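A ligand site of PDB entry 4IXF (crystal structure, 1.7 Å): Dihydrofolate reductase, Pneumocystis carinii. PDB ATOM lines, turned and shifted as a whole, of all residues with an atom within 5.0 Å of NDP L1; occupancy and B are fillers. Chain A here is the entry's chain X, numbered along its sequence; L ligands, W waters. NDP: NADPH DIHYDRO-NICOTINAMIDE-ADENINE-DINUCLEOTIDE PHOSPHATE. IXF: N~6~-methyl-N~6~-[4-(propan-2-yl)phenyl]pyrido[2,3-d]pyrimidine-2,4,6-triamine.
O2A of NDP L1 lies within hydrogen-bond range of OG1 of Thr 61.
N of Lys 60 sits at hydrogen-bond distance from O5B of NDP L1, at 3.2 Å.
N of Arg 59 lies within hydrogen-bond range of O4B of NDP L1.
N of Ser 24 lies within hydrogen-bond range of O3D of NDP L1 (3.5 Å).
The backbone carbonyl oxygen (O) of Ala 12 lies close to a nitrogen (N7N) of NDP L1.
A nitrogen (NAE) of IXF L2 lies within hydrogen-bond range of the backbone carbonyl oxygen (O) of Ile 123 (2.9 Å).
An oxygen (O2D) of NDP L1 sits at hydrogen-bond distance from the backbone carbonyl oxygen (O) of Ser 24, 3.0 Å away.
The backbone NH (N) of Ala 126 is in hydrogen-bond range of an oxygen (O1N) of NDP L1 (3.1 Å).
An oxygen (O2A) of NDP L1 is in hydrogen-bond range of the backbone NH (N) of Thr 61, 2.9 Å away.
N of Gly 125 is in hydrogen-bond range of O2A of NDP L1, at 3.1 Å.
A nitrogen (NAE) of IXF L2 lies within hydrogen-bond range of the backbone carbonyl oxygen (O) of Ile 10 (2.8 Å).
O1X of NDP L1 is in salt-bridge range of NH1 of Arg 59, 2.7 Å away.
OH of Tyr 129 sits at hydrogen-bond distance from NAE of IXF L2 (3.4 Å).
The side-chain hydroxyl (OG1) of Thr 81 sits at hydrogen-bond distance from an oxygen (O2X) of NDP L1, 2.5 Å away.
The backbone NH (N) of Arg 82 is in hydrogen-bond range of an oxygen (O3X) of NDP L1 (2.9 Å).
An oxygen (O1A) of NDP L1 is in hydrogen-bond range of the backbone NH (N) of Leu 128 (3.3 Å).
The backbone NH (N) of Val 11 is in hydrogen-bond range of a nitrogen (N1) of IXF L2 (3.4 Å).
An oxygen (O1N) of NDP L1 sits at hydrogen-bond distance from the backbone NH of Gln 127 (2.9 Å).
O of Ile 80 is in hydrogen-bond range of N of Arg 59 (3.3 Å).
O of Ile 123 sits at hydrogen-bond distance from OH of Tyr 129, at 3.3 Å.
N of Val 154 lies within hydrogen-bond range of O of Gly 20, at 3.3 Å.
The side-chain hydroxyl (OG1) of Thr 81 lies within hydrogen-bond range of the backbone NH (N) of Asn 83, 3.1 Å away.
O of Lys 60 lies close to OD1 of Asn 23 (2.9 Å).
N of Gly 58 is in hydrogen-bond range of O of Gly 124 (2.8 Å).
OG of Ser 64 is in hydrogen-bond range of O of Thr 61, 2.8 Å away.
The side-chain hydroxyl (OG1) of Thr 61 lies within hydrogen-bond range of the backbone NH (N) of Gly 125, 3.0 Å away.
O of Ile 19 lies close to O7N of NDP L1 (3.1 Å).
An oxygen (O4B) of NDP L1 lies close to the backbone carbonyl oxygen (O) of Ile 80 (3.3 Å).
CA of Val 11 touches N7N of NDP L1, 3.5 Å away.
Gly 20 touches NDP L1.
Arg 21 touches NDP L1.
ND2 of Asn 23 touches C3D of NDP L1 (3.5 Å).
Leu 25 touches NDP L1.
Trp 27 touches NDP L1 (CZ2 to O7N, 3.4 Å).
CA of Gly 58 touches O2A of NDP L1 (3.4 Å).
Lys 96 touches NDP L1.
Ile 123 touches NDP L1.
CA of Gly 124 touches C5N of NDP L1, 3.7 Å away.
Tyr 129 touches NDP L1.
CB of Ala 131 touches N6A of NDP L1 (3.4 Å).
Val 154 touches NDP L1.
Hydrophobic or aromatic side chains that line NDP L1: Val 11, Ala 12, Ile 19, Leu 25, Trp 27, Ile 80, Ala 126, Leu 128, Ala 131 and Val 154.
Along chain A the residues within 4 Å of NDP L1 span positions 11 to 154.
Water W4 bridges an oxygen (O3X) of NDP L1 (2.6 Å) and the guanidinium group of Arg 82 (3.4 Å).
Water W5 bridges a nitrogen (N1A) of NDP L1 and the guanidinium group of Arg 82.
Water W1 bridges an oxygen (O2D) of NDP L1 (2.7 Å) and the side-chain hydroxyl (OG) of Ser 64 (2.7 Å).
Water W6 lies within hydrogen-bond range of the backbone NH (N) of Asn 23 (2.7 Å) and an oxygen (O3D) of NDP L1 (3.3 Å).
Water W7 lies within hydrogen-bond range of the backbone carbonyl oxygen (O) of Gln 127 (2.8 Å) and a nitrogen (N6A) of NDP L1 (3.4 Å).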
ATOM      1  N   ILE A  10       7.276   5.160 -12.849  1.00  0.00           N
ATOM      2  CA  ILE A  10       7.381   3.802 -13.454  1.00  0.00           C
ATOM      3  C   ILE A  10       7.963   3.996 -14.865  1.00  0.00           C
ATOM      4  O   ILE A  10       7.581   4.935 -15.611  1.00  0.00           O
ATOM      5  CB  ILE A  10       6.014   3.063 -13.494  1.00  0.00           C
ATOM      6  CG1 ILE A  10       6.143   1.641 -14.191  1.00  0.00           C
ATOM      7  CG2 ILE A  10       4.886   3.890 -14.180  1.00  0.00           C
ATOM      8  CD1 ILE A  10       5.074   0.671 -13.731  1.00  0.00           C
ATOM      9  N   VAL A  11       8.876   3.111 -15.190  1.00  0.00           N
ATOM     10  CA  VAL A  11       9.705   3.242 -16.419  1.00  0.00           C
ATOM     11  C   VAL A  11      10.211   1.891 -16.852  1.00  0.00           C
ATOM     12  O   VAL A  11      10.540   1.082 -16.003  1.00  0.00           O
ATOM     13  CB  VAL A  11      10.907   4.263 -16.147  1.00  0.00           C
ATOM     14  CG1 VAL A  11      11.917   3.764 -15.080  1.00  0.00           C
ATOM     15  CG2 VAL A  11      11.646   4.631 -17.461  1.00  0.00           C
ATOM     16  N   ALA A  12      10.440   1.738 -18.158  1.00  0.00           N
ATOM     17  CA  ALA A  12      11.126   0.596 -18.712  1.00  0.00           C
ATOM     18  C   ALA A  12      12.314   1.211 -19.433  1.00  0.00           C
ATOM     19  O   ALA A  12      12.174   2.246 -20.190  1.00  0.00           O
ATOM     20  CB  ALA A  12      10.229  -0.150 -19.692  1.00  0.00           C
ATOM     21  N   LEU A  13      13.466   0.741 -19.045  1.00  0.00           N
ATOM     22  CA  LEU A  13      14.723   1.297 -19.561  1.00  0.00           C
ATOM     23  C   LEU A  13      15.790   0.285 -19.869  1.00  0.00           C
ATOM     24  O   LEU A  13      15.939  -0.723 -19.180  1.00  0.00           O
ATOM     25  CB  LEU A  13      15.271   2.421 -18.644  1.00  0.00           C
ATOM     26  CG  LEU A  13      16.040   2.101 -17.379  1.00  0.00           C
ATOM     27  CD1 LEU A  13      16.365   3.447 -16.692  1.00  0.00           C
ATOM     28  CD2 LEU A  13      15.206   1.299 -16.412  1.00  0.00           C
ATOM     29  N   ILE A  19      15.171   5.056 -23.136  1.00  0.00           N
ATOM     30  CA  ILE A  19      13.666   4.894 -22.953  1.00  0.00           C
ATOM     31  C   ILE A  19      12.789   5.015 -24.180  1.00  0.00           C
ATOM     32  O   ILE A  19      11.654   4.598 -24.167  1.00  0.00           O
ATOM     33  CB  ILE A  19      13.106   5.755 -21.769  1.00  0.00           C
ATOM     34  CG1 ILE A  19      13.249   7.286 -22.015  1.00  0.00           C
ATOM     35  CG2 ILE A  19      13.849   5.328 -20.462  1.00  0.00           C
ATOM     36  CD1 ILE A  19      12.448   8.194 -21.103  1.00  0.00           C
ATOM     37  N   GLY A  20      13.284   5.634 -25.282  1.00  0.00           N
ATOM     38  CA  GLY A  20      12.385   5.861 -26.374  1.00  0.00           C
ATOM     39  C   GLY A  20      13.165   6.092 -27.672  1.00  0.00           C
ATOM     40  O   GLY A  20      14.399   6.277 -27.679  1.00  0.00           O
ATOM     41  N   ARG A  21      12.422   5.991 -28.769  1.00  0.00           N
ATOM     42  CA  ARG A  21      13.048   6.184 -30.114  1.00  0.00           C
ATOM     43  C   ARG A  21      11.921   6.609 -31.036  1.00  0.00           C
ATOM     44  O   ARG A  21      10.822   5.990 -31.032  1.00  0.00           O
ATOM     45  CB  ARG A  21      13.604   4.852 -30.572  1.00  0.00           C
ATOM     46  CG  ARG A  21      14.167   4.833 -31.998  1.00  0.00           C
ATOM     47  CD  ARG A  21      14.822   3.470 -32.246  1.00  0.00           C
ATOM     48  NE  ARG A  21      15.457   3.332 -33.571  1.00  0.00           N
ATOM     49  CZ  ARG A  21      15.952   4.355 -34.265  1.00  0.00           C
ATOM     50  NH1 ARG A  21      15.933   5.582 -33.730  1.00  0.00           N
ATOM     51  NH2 ARG A  21      16.503   4.136 -35.462  1.00  0.00           N
ATOM     52  N   ASN A  23       9.771   9.044 -31.053  1.00  0.00           N
ATOM     53  CA  ASN A  23       8.557   9.186 -30.218  1.00  0.00           C
ATOM     54  C   ASN A  23       7.678   7.939 -29.958  1.00  0.00           C
ATOM     55  O   ASN A  23       6.442   8.059 -29.791  1.00  0.00           O
ATOM     56  CB  ASN A  23       7.682  10.447 -30.602  1.00  0.00           C
ATOM     57  CG  ASN A  23       6.956  11.076 -29.378  1.00  0.00           C
ATOM     58  OD1 ASN A  23       5.682  11.148 -29.298  1.00  0.00           O
ATOM     59  ND2 ASN A  23       7.759  11.550 -28.414  1.00  0.00           N
ATOM     60  N   SER A  24       8.291   6.764 -29.867  1.00  0.00           N
ATOM     61  CA  SER A  24       7.625   5.620 -29.237  1.00  0.00           C
ATOM     62  C   SER A  24       8.600   4.729 -28.489  1.00  0.00           C
ATOM     63  O   SER A  24       9.696   5.137 -28.134  1.00  0.00           O
ATOM     64  CB  SER A  24       6.808   4.775 -30.235  1.00  0.00           C
ATOM     65  OG  SER A  24       7.645   4.527 -31.334  1.00  0.00           O
ATOM     66  N   LEU A  25       8.200   3.498 -28.261  1.00  0.00           N
ATOM     67  CA  LEU A  25       9.042   2.591 -27.467  1.00  0.00           C
ATOM     68  C   LEU A  25       9.827   1.746 -28.416  1.00  0.00           C
ATOM     69  O   LEU A  25       9.248   1.248 -29.389  1.00  0.00           O
ATOM     70  CB  LEU A  25       8.129   1.675 -26.616  1.00  0.00           C
ATOM     71  CG  LEU A  25       7.164   2.388 -25.692  1.00  0.00           C
ATOM     72  CD1 LEU A  25       6.228   1.382 -25.060  1.00  0.00           C
ATOM     73  CD2 LEU A  25       8.021   3.116 -24.647  1.00  0.00           C
ATOM     74  N   TRP A  27      10.775  -1.260 -28.342  1.00  0.00           N
ATOM     75  CA  TRP A  27      10.551  -2.651 -28.216  1.00  0.00           C
ATOM     76  C   TRP A  27       9.045  -2.777 -28.222  1.00  0.00           C
ATOM     77  O   TRP A  27       8.315  -1.780 -28.114  1.00  0.00           O
ATOM     78  CB  TRP A  27      11.144  -3.161 -26.910  1.00  0.00           C
ATOM     79  CG  TRP A  27      10.764  -2.262 -25.715  1.00  0.00           C
ATOM     80  CD1 TRP A  27       9.522  -2.162 -25.067  1.00  0.00           C
ATOM     81  CD2 TRP A  27      11.625  -1.271 -25.067  1.00  0.00           C
ATOM     82  NE1 TRP A  27       9.582  -1.227 -24.039  1.00  0.00           N
ATOM     83  CE2 TRP A  27      10.822  -0.644 -24.001  1.00  0.00           C
ATOM     84  CE3 TRP A  27      12.936  -0.874 -25.255  1.00  0.00           C
ATOM     85  CZ2 TRP A  27      11.350   0.348 -23.174  1.00  0.00           C
ATOM     86  CZ3 TRP A  27      13.482   0.128 -24.406  1.00  0.00           C
ATOM     87  CH2 TRP A  27      12.692   0.731 -23.411  1.00  0.00           C
ATOM     88  N   GLY A  58       3.977  13.567 -19.758  1.00  0.00           N
ATOM     89  CA  GLY A  58       4.341  14.700 -20.650  1.00  0.00           C
ATOM     90  C   GLY A  58       3.483  14.681 -21.904  1.00  0.00           C
ATOM     91  O   GLY A  58       2.914  13.611 -22.287  1.00  0.00           O
ATOM     92  N   ARG A  59       3.424  15.866 -22.564  1.00  0.00           N
ATOM     93  CA  ARG A  59       2.658  16.010 -23.779  1.00  0.00           C
ATOM     94  C   ARG A  59       3.152  15.021 -24.846  1.00  0.00           C
ATOM     95  O   ARG A  59       2.338  14.431 -25.496  1.00  0.00           O
ATOM     96  CB  ARG A  59       2.708  17.445 -24.312  1.00  0.00           C
ATOM     97  CG  ARG A  59       1.607  17.642 -25.365  1.00  0.00           C
ATOM     98  CD  ARG A  59       2.109  18.312 -26.624  1.00  0.00           C
ATOM     99  NE  ARG A  59       3.343  19.093 -26.515  1.00  0.00           N
ATOM    100  CZ  ARG A  59       4.297  19.021 -27.432  1.00  0.00           C
ATOM    101  NH1 ARG A  59       5.430  19.737 -27.336  1.00  0.00           N
ATOM    102  NH2 ARG A  59       4.136  18.172 -28.435  1.00  0.00           N
ATOM    103  N   LYS A  60       4.477  14.855 -25.017  1.00  0.00           N
ATOM    104  CA  LYS A  60       4.973  13.940 -26.110  1.00  0.00           C
ATOM    105  C   LYS A  60       4.613  12.463 -25.842  1.00  0.00           C
ATOM    106  O   LYS A  60       4.278  11.683 -26.778  1.00  0.00           O
ATOM    107  CB  LYS A  60       6.457  14.116 -26.385  1.00  0.00           C
ATOM    108  CG  LYS A  60       6.821  15.549 -26.806  1.00  0.00           C
ATOM    109  CD  LYS A  60       8.300  15.660 -27.106  1.00  0.00           C
ATOM    110  CE  LYS A  60       8.651  17.064 -27.611  1.00  0.00           C
ATOM    111  NZ  LYS A  60      10.115  17.100 -27.906  1.00  0.00           N
ATOM    112  N   THR A  61       4.669  12.064 -24.562  1.00  0.00           N
ATOM    113  CA  THR A  61       4.162  10.739 -24.168  1.00  0.00           C
ATOM    114  C   THR A  61       2.690  10.602 -24.464  1.00  0.00           C
ATOM    115  O   THR A  61       2.251   9.521 -24.945  1.00  0.00           O
ATOM    116  CB  THR A  61       4.486  10.418 -22.696  1.00  0.00           C
ATOM    117  OG1 THR A  61       5.899  10.412 -22.586  1.00  0.00           O
ATOM    118  CG2 THR A  61       3.918   9.042 -22.261  1.00  0.00           C
ATOM    119  N   SER A  64       2.352   9.851 -28.026  1.00  0.00           N
ATOM    120  CA  SER A  64       2.911   8.536 -28.351  1.00  0.00           C
ATOM    121  C   SER A  64       1.936   7.399 -28.104  1.00  0.00           C
ATOM    122  O   SER A  64       2.176   6.276 -28.601  1.00  0.00           O
ATOM    123  CB  SER A  64       4.203   8.297 -27.573  1.00  0.00           C
ATOM    124  OG  SER A  64       3.902   7.755 -26.266  1.00  0.00           O
ATOM    125  N   ILE A  80       0.856  16.939 -18.697  1.00  0.00           N
ATOM    126  CA  ILE A  80       1.642  18.104 -18.287  1.00  0.00           C
ATOM    127  C   ILE A  80       2.157  18.850 -19.550  1.00  0.00           C
ATOM    128  O   ILE A  80       2.928  18.287 -20.383  1.00  0.00           O
ATOM    129  CB  ILE A  80       2.876  17.706 -17.464  1.00  0.00           C
ATOM    130  CG1 ILE A  80       2.477  16.786 -16.270  1.00  0.00           C
ATOM    131  CG2 ILE A  80       3.568  18.961 -16.907  1.00  0.00           C
ATOM    132  CD1 ILE A  80       1.278  17.274 -15.494  1.00  0.00           C
ATOM    133  N   THR A  81       1.775  20.119 -19.683  1.00  0.00           N
ATOM    134  CA  THR A  81       2.255  20.890 -20.867  1.00  0.00           C
ATOM    135  C   THR A  81       2.310  22.363 -20.481  1.00  0.00           C
ATOM    136  O   THR A  81       1.493  22.795 -19.701  1.00  0.00           O
ATOM    137  CB  THR A  81       1.284  20.738 -22.100  1.00  0.00           C
ATOM    138  OG1 THR A  81       1.571  21.743 -23.109  1.00  0.00           O
ATOM    139  CG2 THR A  81      -0.214  20.807 -21.701  1.00  0.00           C
ATOM    140  N   ARG A  82       3.198  23.154 -21.060  1.00  0.00           N
ATOM    141  CA  ARG A  82       3.245  24.571 -20.759  1.00  0.00           C
ATOM    142  C   ARG A  82       2.431  25.397 -21.716  1.00  0.00           C
ATOM    143  O   ARG A  82       2.553  26.588 -21.723  1.00  0.00           O
ATOM    144  CB  ARG A  82       4.663  25.071 -20.789  1.00  0.00           C
ATOM    145  CG  ARG A  82       5.590  24.379 -19.853  1.00  0.00           C
ATOM    146  CD  ARG A  82       6.871  25.129 -19.651  1.00  0.00           C
ATOM    147  NE  ARG A  82       7.963  24.204 -19.628  1.00  0.00           N
ATOM    148  CZ  ARG A  82       8.567  23.856 -18.522  1.00  0.00           C
ATOM    149  NH1 ARG A  82       8.166  24.407 -17.401  1.00  0.00           N
ATOM    150  NH2 ARG A  82       9.534  22.992 -18.538  1.00  0.00           N
ATOM    151  N   ASN A  83       1.605  24.738 -22.522  1.00  0.00           N
ATOM    152  CA  ASN A  83       0.788  25.427 -23.518  1.00  0.00           C
ATOM    153  C   ASN A  83      -0.700  25.223 -23.286  1.00  0.00           C
ATOM    154  O   ASN A  83      -1.284  24.248 -23.775  1.00  0.00           O
ATOM    155  CB  ASN A  83       1.169  24.984 -24.927  1.00  0.00           C
ATOM    156  CG  ASN A  83       0.406  25.732 -26.004  1.00  0.00           C
ATOM    157  OD1 ASN A  83      -0.519  26.485 -25.708  1.00  0.00           O
ATOM    158  ND2 ASN A  83       0.786  25.522 -27.258  1.00  0.00           N
ATOM    159  N   LYS A  96       0.234  22.733 -15.933  1.00  0.00           N
ATOM    160  CA  LYS A  96       1.483  23.259 -16.452  1.00  0.00           C
ATOM    161  C   LYS A  96       2.691  22.815 -15.695  1.00  0.00           C
ATOM    162  O   LYS A  96       3.798  23.216 -16.014  1.00  0.00           O
ATOM    163  CB  LYS A  96       1.437  24.804 -16.595  1.00  0.00           C
ATOM    164  CG  LYS A  96       0.758  25.600 -15.518  1.00  0.00           C
ATOM    165  CD  LYS A  96       0.671  27.049 -16.023  1.00  0.00           C
ATOM    166  CE  LYS A  96       0.351  28.067 -14.946  1.00  0.00           C
ATOM    167  NZ  LYS A  96       0.762  29.440 -15.407  1.00  0.00           N
ATOM    168  N   SER A  97       2.505  21.983 -14.686  1.00  0.00           N
ATOM    169  CA  SER A  97       3.579  21.430 -13.898  1.00  0.00           C
ATOM    170  C   SER A  97       3.072  20.254 -13.073  1.00  0.00           C
ATOM    171  O   SER A  97       1.885  20.066 -12.900  1.00  0.00           O
ATOM    172  CB  SER A  97       4.227  22.472 -12.935  1.00  0.00           C
ATOM    173  OG  SER A  97       3.420  22.732 -11.792  1.00  0.00           O
ATOM    174  N   ILE A 123       4.547   8.573 -15.502  1.00  0.00           N
ATOM    175  CA  ILE A 123       4.731   7.449 -16.468  1.00  0.00           C
ATOM    176  C   ILE A 123       5.592   7.868 -17.676  1.00  0.00           C
ATOM    177  O   ILE A 123       5.724   7.102 -18.655  1.00  0.00           O
ATOM    178  CB  ILE A 123       3.388   6.834 -16.960  1.00  0.00           C
ATOM    179  CG1 ILE A 123       2.600   7.856 -17.802  1.00  0.00           C
ATOM    180  CG2 ILE A 123       2.560   6.335 -15.764  1.00  0.00           C
ATOM    181  CD1 ILE A 123       1.547   7.240 -18.739  1.00  0.00           C
ATOM    182  N   GLY A 124       6.235   9.044 -17.571  1.00  0.00           N
ATOM    183  CA  GLY A 124       7.137   9.538 -18.630  1.00  0.00           C
ATOM    184  C   GLY A 124       6.671  10.848 -19.322  1.00  0.00           C
ATOM    185  O   GLY A 124       5.594  11.372 -18.995  1.00  0.00           O
ATOM    186  N   GLY A 125       7.465  11.408 -20.257  1.00  0.00           N
ATOM    187  CA  GLY A 125       8.735  10.837 -20.729  1.00  0.00           C
ATOM    188  C   GLY A 125       9.920  11.432 -20.032  1.00  0.00           C
ATOM    189  O   GLY A 125       9.819  11.822 -18.881  1.00  0.00           O
ATOM    190  N   ALA A 126      11.073  11.488 -20.699  1.00  0.00           N
ATOM    191  CA  ALA A 126      12.246  12.024 -20.037  1.00  0.00           C
ATOM    192  C   ALA A 126      12.090  13.414 -19.425  1.00  0.00           C
ATOM    193  O   ALA A 126      12.597  13.610 -18.346  1.00  0.00           O
ATOM    194  CB  ALA A 126      13.437  11.983 -20.989  1.00  0.00           C
ATOM    195  N   GLN A 127      11.409  14.328 -20.052  1.00  0.00           N
ATOM    196  CA  GLN A 127      11.376  15.645 -19.493  1.00  0.00           C
ATOM    197  C   GLN A 127      10.578  15.640 -18.193  1.00  0.00           C
ATOM    198  O   GLN A 127      10.979  16.195 -17.234  1.00  0.00           O
ATOM    199  CB  GLN A 127      10.820  16.643 -20.484  1.00  0.00           C
ATOM    200  CG  GLN A 127      10.876  18.038 -19.962  1.00  0.00           C
ATOM    201  CD  GLN A 127      10.561  19.068 -21.018  1.00  0.00           C
ATOM    202  OE1 GLN A 127      10.039  20.109 -20.706  1.00  0.00           O
ATOM    203  NE2 GLN A 127      10.883  18.772 -22.243  1.00  0.00           N
ATOM    204  N   LEU A 128       9.432  14.984 -18.225  1.00  0.00           N
ATOM    205  CA  LEU A 128       8.659  14.865 -17.001  1.00  0.00           C
ATOM    206  C   LEU A 128       9.347  14.023 -15.926  1.00  0.00           C
ATOM    207  O   LEU A 128       9.205  14.336 -14.723  1.00  0.00           O
ATOM    208  CB  LEU A 128       7.255  14.302 -17.305  1.00  0.00           C
ATOM    209  CG  LEU A 128       6.063  14.767 -16.479  1.00  0.00           C
ATOM    210  CD1 LEU A 128       4.957  13.776 -16.235  1.00  0.00           C
ATOM    211  CD2 LEU A 128       6.201  15.878 -15.442  1.00  0.00           C
ATOM    212  N   TYR A 129      10.114  13.016 -16.343  1.00  0.00           N
ATOM    213  CA  TYR A 129      10.795  12.169 -15.390  1.00  0.00           C
ATOM    214  C   TYR A 129      11.874  13.040 -14.717  1.00  0.00           C
ATOM    215  O   TYR A 129      12.184  12.887 -13.558  1.00  0.00           O
ATOM    216  CB  TYR A 129      11.561  11.049 -16.046  1.00  0.00           C
ATOM    217  CG  TYR A 129      10.742   9.818 -16.433  1.00  0.00           C
ATOM    218  CD1 TYR A 129       9.694   9.352 -15.609  1.00  0.00           C
ATOM    219  CD2 TYR A 129      11.087   9.126 -17.568  1.00  0.00           C
ATOM    220  CE1 TYR A 129       9.002   8.148 -16.002  1.00  0.00           C
ATOM    221  CE2 TYR A 129      10.421   7.963 -17.946  1.00  0.00           C
ATOM    222  CZ  TYR A 129       9.334   7.526 -17.154  1.00  0.00           C
ATOM    223  OH  TYR A 129       8.718   6.342 -17.619  1.00  0.00           O
ATOM    224  N   ALA A 131      11.716  16.341 -13.961  1.00  0.00           N
ATOM    225  CA  ALA A 131      10.947  17.086 -12.965  1.00  0.00           C
ATOM    226  C   ALA A 131      10.580  16.158 -11.779  1.00  0.00           C
ATOM    227  O   ALA A 131      10.713  16.576 -10.633  1.00  0.00           O
ATOM    228  CB  ALA A 131       9.672  17.661 -13.560  1.00  0.00           C
ATOM    229  N   VAL A 154      16.017   8.981 -26.742  1.00  0.00           N
ATOM    230  CA  VAL A 154      15.624   9.713 -25.569  1.00  0.00           C
ATOM    231  C   VAL A 154      16.023   8.804 -24.386  1.00  0.00           C
ATOM    232  O   VAL A 154      15.914   7.568 -24.472  1.00  0.00           O
ATOM    233  CB  VAL A 154      14.101  10.018 -25.591  1.00  0.00           C
ATOM    234  CG1 VAL A 154      13.576  10.365 -24.213  1.00  0.00           C
ATOM    235  CG2 VAL A 154      13.820  11.202 -26.524  1.00  0.00           C
HETATM  236  PA  NDP L   1       7.679  13.996 -22.536  1.00  0.00           P
HETATM  237  O1A NDP L   1       8.447  14.299 -21.264  1.00  0.00           O
HETATM  238  O2A NDP L   1       6.573  13.063 -22.662  1.00  0.00           O
HETATM  239  O5B NDP L   1       7.008  15.397 -23.183  1.00  0.00           O
HETATM  240  C5B NDP L   1       7.755  16.613 -22.975  1.00  0.00           C
HETATM  241  C4B NDP L   1       6.760  17.714 -23.098  1.00  0.00           C
HETATM  242  O4B NDP L   1       5.764  17.590 -22.016  1.00  0.00           O
HETATM  243  C3B NDP L   1       7.429  19.112 -22.988  1.00  0.00           C
HETATM  244  O3B NDP L   1       7.648  19.617 -24.335  1.00  0.00           O
HETATM  245  C2B NDP L   1       6.302  19.866 -22.319  1.00  0.00           C
HETATM  246  O2B NDP L   1       5.177  20.011 -23.117  1.00  0.00           O
HETATM  247  C1B NDP L   1       5.796  18.841 -21.263  1.00  0.00           C
HETATM  248  N9A NDP L   1       6.562  18.753 -20.025  1.00  0.00           N
HETATM  249  C8A NDP L   1       7.385  17.763 -19.620  1.00  0.00           C
HETATM  250  N7A NDP L   1       7.909  18.032 -18.435  1.00  0.00           N
HETATM  251  C5A NDP L   1       7.335  19.203 -18.029  1.00  0.00           C
HETATM  252  C6A NDP L   1       7.434  19.990 -16.884  1.00  0.00           C
HETATM  253  N6A NDP L   1       8.202  19.650 -15.832  1.00  0.00           N
HETATM  254  N1A NDP L   1       6.719  21.131 -16.846  1.00  0.00           N
HETATM  255  C2A NDP L   1       5.923  21.542 -17.847  1.00  0.00           C
HETATM  256  N3A NDP L   1       5.798  20.828 -18.959  1.00  0.00           N
HETATM  257  C4A NDP L   1       6.508  19.674 -19.059  1.00  0.00           C
HETATM  258  O3  NDP L   1       8.688  13.817 -23.745  1.00  0.00           O
HETATM  259  PN  NDP L   1      10.081  13.277 -23.952  1.00  0.00           P
HETATM  260  O1N NDP L   1      11.083  13.660 -22.903  1.00  0.00           O
HETATM  261  O2N NDP L   1      10.498  13.560 -25.413  1.00  0.00           O
HETATM  262  O5D NDP L   1       9.954  11.750 -23.915  1.00  0.00           O
HETATM  263  C5D NDP L   1       8.960  11.014 -24.763  1.00  0.00           C
HETATM  264  C4D NDP L   1       9.661   9.767 -25.322  1.00  0.00           C
HETATM  265  O4D NDP L   1       9.713   8.950 -24.118  1.00  0.00           O
HETATM  266  C3D NDP L   1       8.934   8.907 -26.372  1.00  0.00           C
HETATM  267  O3D NDP L   1       9.904   8.129 -27.088  1.00  0.00           O
HETATM  268  C2D NDP L   1       8.159   7.927 -25.532  1.00  0.00           C
HETATM  269  O2D NDP L   1       7.900   6.698 -26.245  1.00  0.00           O
HETATM  270  C1D NDP L   1       9.146   7.618 -24.425  1.00  0.00           C
HETATM  271  N1N NDP L   1       8.555   7.030 -23.170  1.00  0.00           N
HETATM  272  C2N NDP L   1       9.192   5.852 -22.695  1.00  0.00           C
HETATM  273  C3N NDP L   1       8.767   5.274 -21.514  1.00  0.00           C
HETATM  274  C7N NDP L   1       9.425   3.927 -21.046  1.00  0.00           C
HETATM  275  O7N NDP L   1      10.253   3.263 -21.749  1.00  0.00           O
HETATM  276  N7N NDP L   1       9.031   3.601 -19.836  1.00  0.00           N
HETATM  277  C4N NDP L   1       7.627   5.823 -20.869  1.00  0.00           C
HETATM  278  C5N NDP L   1       7.040   7.004 -21.339  1.00  0.00           C
HETATM  279  C6N NDP L   1       7.505   7.626 -22.504  1.00  0.00           C
HETATM  280  P2B NDP L   1       4.835  21.352 -24.137  1.00  0.00           P
HETATM  281  O1X NDP L   1       5.962  21.243 -25.169  1.00  0.00           O
HETATM  282  O2X NDP L   1       3.447  21.088 -24.613  1.00  0.00           O
HETATM  283  O3X NDP L   1       5.099  22.682 -23.205  1.00  0.00           O
HETATM  284  CAA IXF L   2      -2.228   1.419 -24.317  1.00  0.00           C
HETATM  285  CAV IXF L   2      -0.921   1.275 -25.142  1.00  0.00           C
HETATM  286  CAB IXF L   2      -0.586  -0.198 -25.439  1.00  0.00           C
HETATM  287  CAQ IXF L   2       0.293   1.969 -24.426  1.00  0.00           C
HETATM  288  CAG IXF L   2       1.219   2.675 -25.188  1.00  0.00           C
HETATM  289  CAI IXF L   2       2.323   3.321 -24.576  1.00  0.00           C
HETATM  290  CAF IXF L   2       0.501   1.902 -23.040  1.00  0.00           C
HETATM  291  CAH IXF L   2       1.589   2.539 -22.461  1.00  0.00           C
HETATM  292  CAR IXF L   2       2.535   3.240 -23.201  1.00  0.00           C
HETATM  293  NAW IXF L   2       3.650   3.815 -22.552  1.00  0.00           N
HETATM  294  CAC IXF L   2       3.860   5.255 -22.505  1.00  0.00           C
HETATM  295  CAS IXF L   2       4.364   3.009 -21.704  1.00  0.00           C
HETATM  296  CAK IXF L   2       4.886   3.535 -20.473  1.00  0.00           C
HETATM  297  C5  IXF L   2       5.571   2.665 -19.642  1.00  0.00           C
HETATM  298  C6  IXF L   2       6.139   3.063 -18.374  1.00  0.00           C
HETATM  299  NAE IXF L   2       6.022   4.336 -17.896  1.00  0.00           N
HETATM  300  N1  IXF L   2       6.712   2.122 -17.649  1.00  0.00           N
HETATM  301  C2  IXF L   2       6.829   0.823 -18.017  1.00  0.00           C
HETATM  302  NAD IXF L   2       7.443  -0.146 -17.270  1.00  0.00           N
HETATM  303  N3  IXF L   2       6.354   0.443 -19.225  1.00  0.00           N
HETATM  304  C4  IXF L   2       5.696   1.303 -20.024  1.00  0.00           C
HETATM  305  NAL IXF L   2       5.203   0.788 -21.211  1.00  0.00           N
HETATM  306  CAJ IXF L   2       4.559   1.651 -22.008  1.00  0.00           C
HETATM  307  O   HOH W   1       5.501   5.627 -25.662  1.00  0.00           O
HETATM  308  O   HOH W   2       6.868  19.946 -13.299  1.00  0.00           O
HETATM  309  O   HOH W   3      13.608  14.685 -23.487  1.00  0.00           O
HETATM  310  O   HOH W   4       7.610  23.262 -22.831  1.00  0.00           O
HETATM  311  O   HOH W   5       7.141  22.768 -14.783  1.00  0.00           O
HETATM  312  O   HOH W   6      11.651   9.941 -29.272  1.00  0.00           O
HETATM  313  O   HOH W   7      11.393  18.879 -16.800  1.00  0.00           O
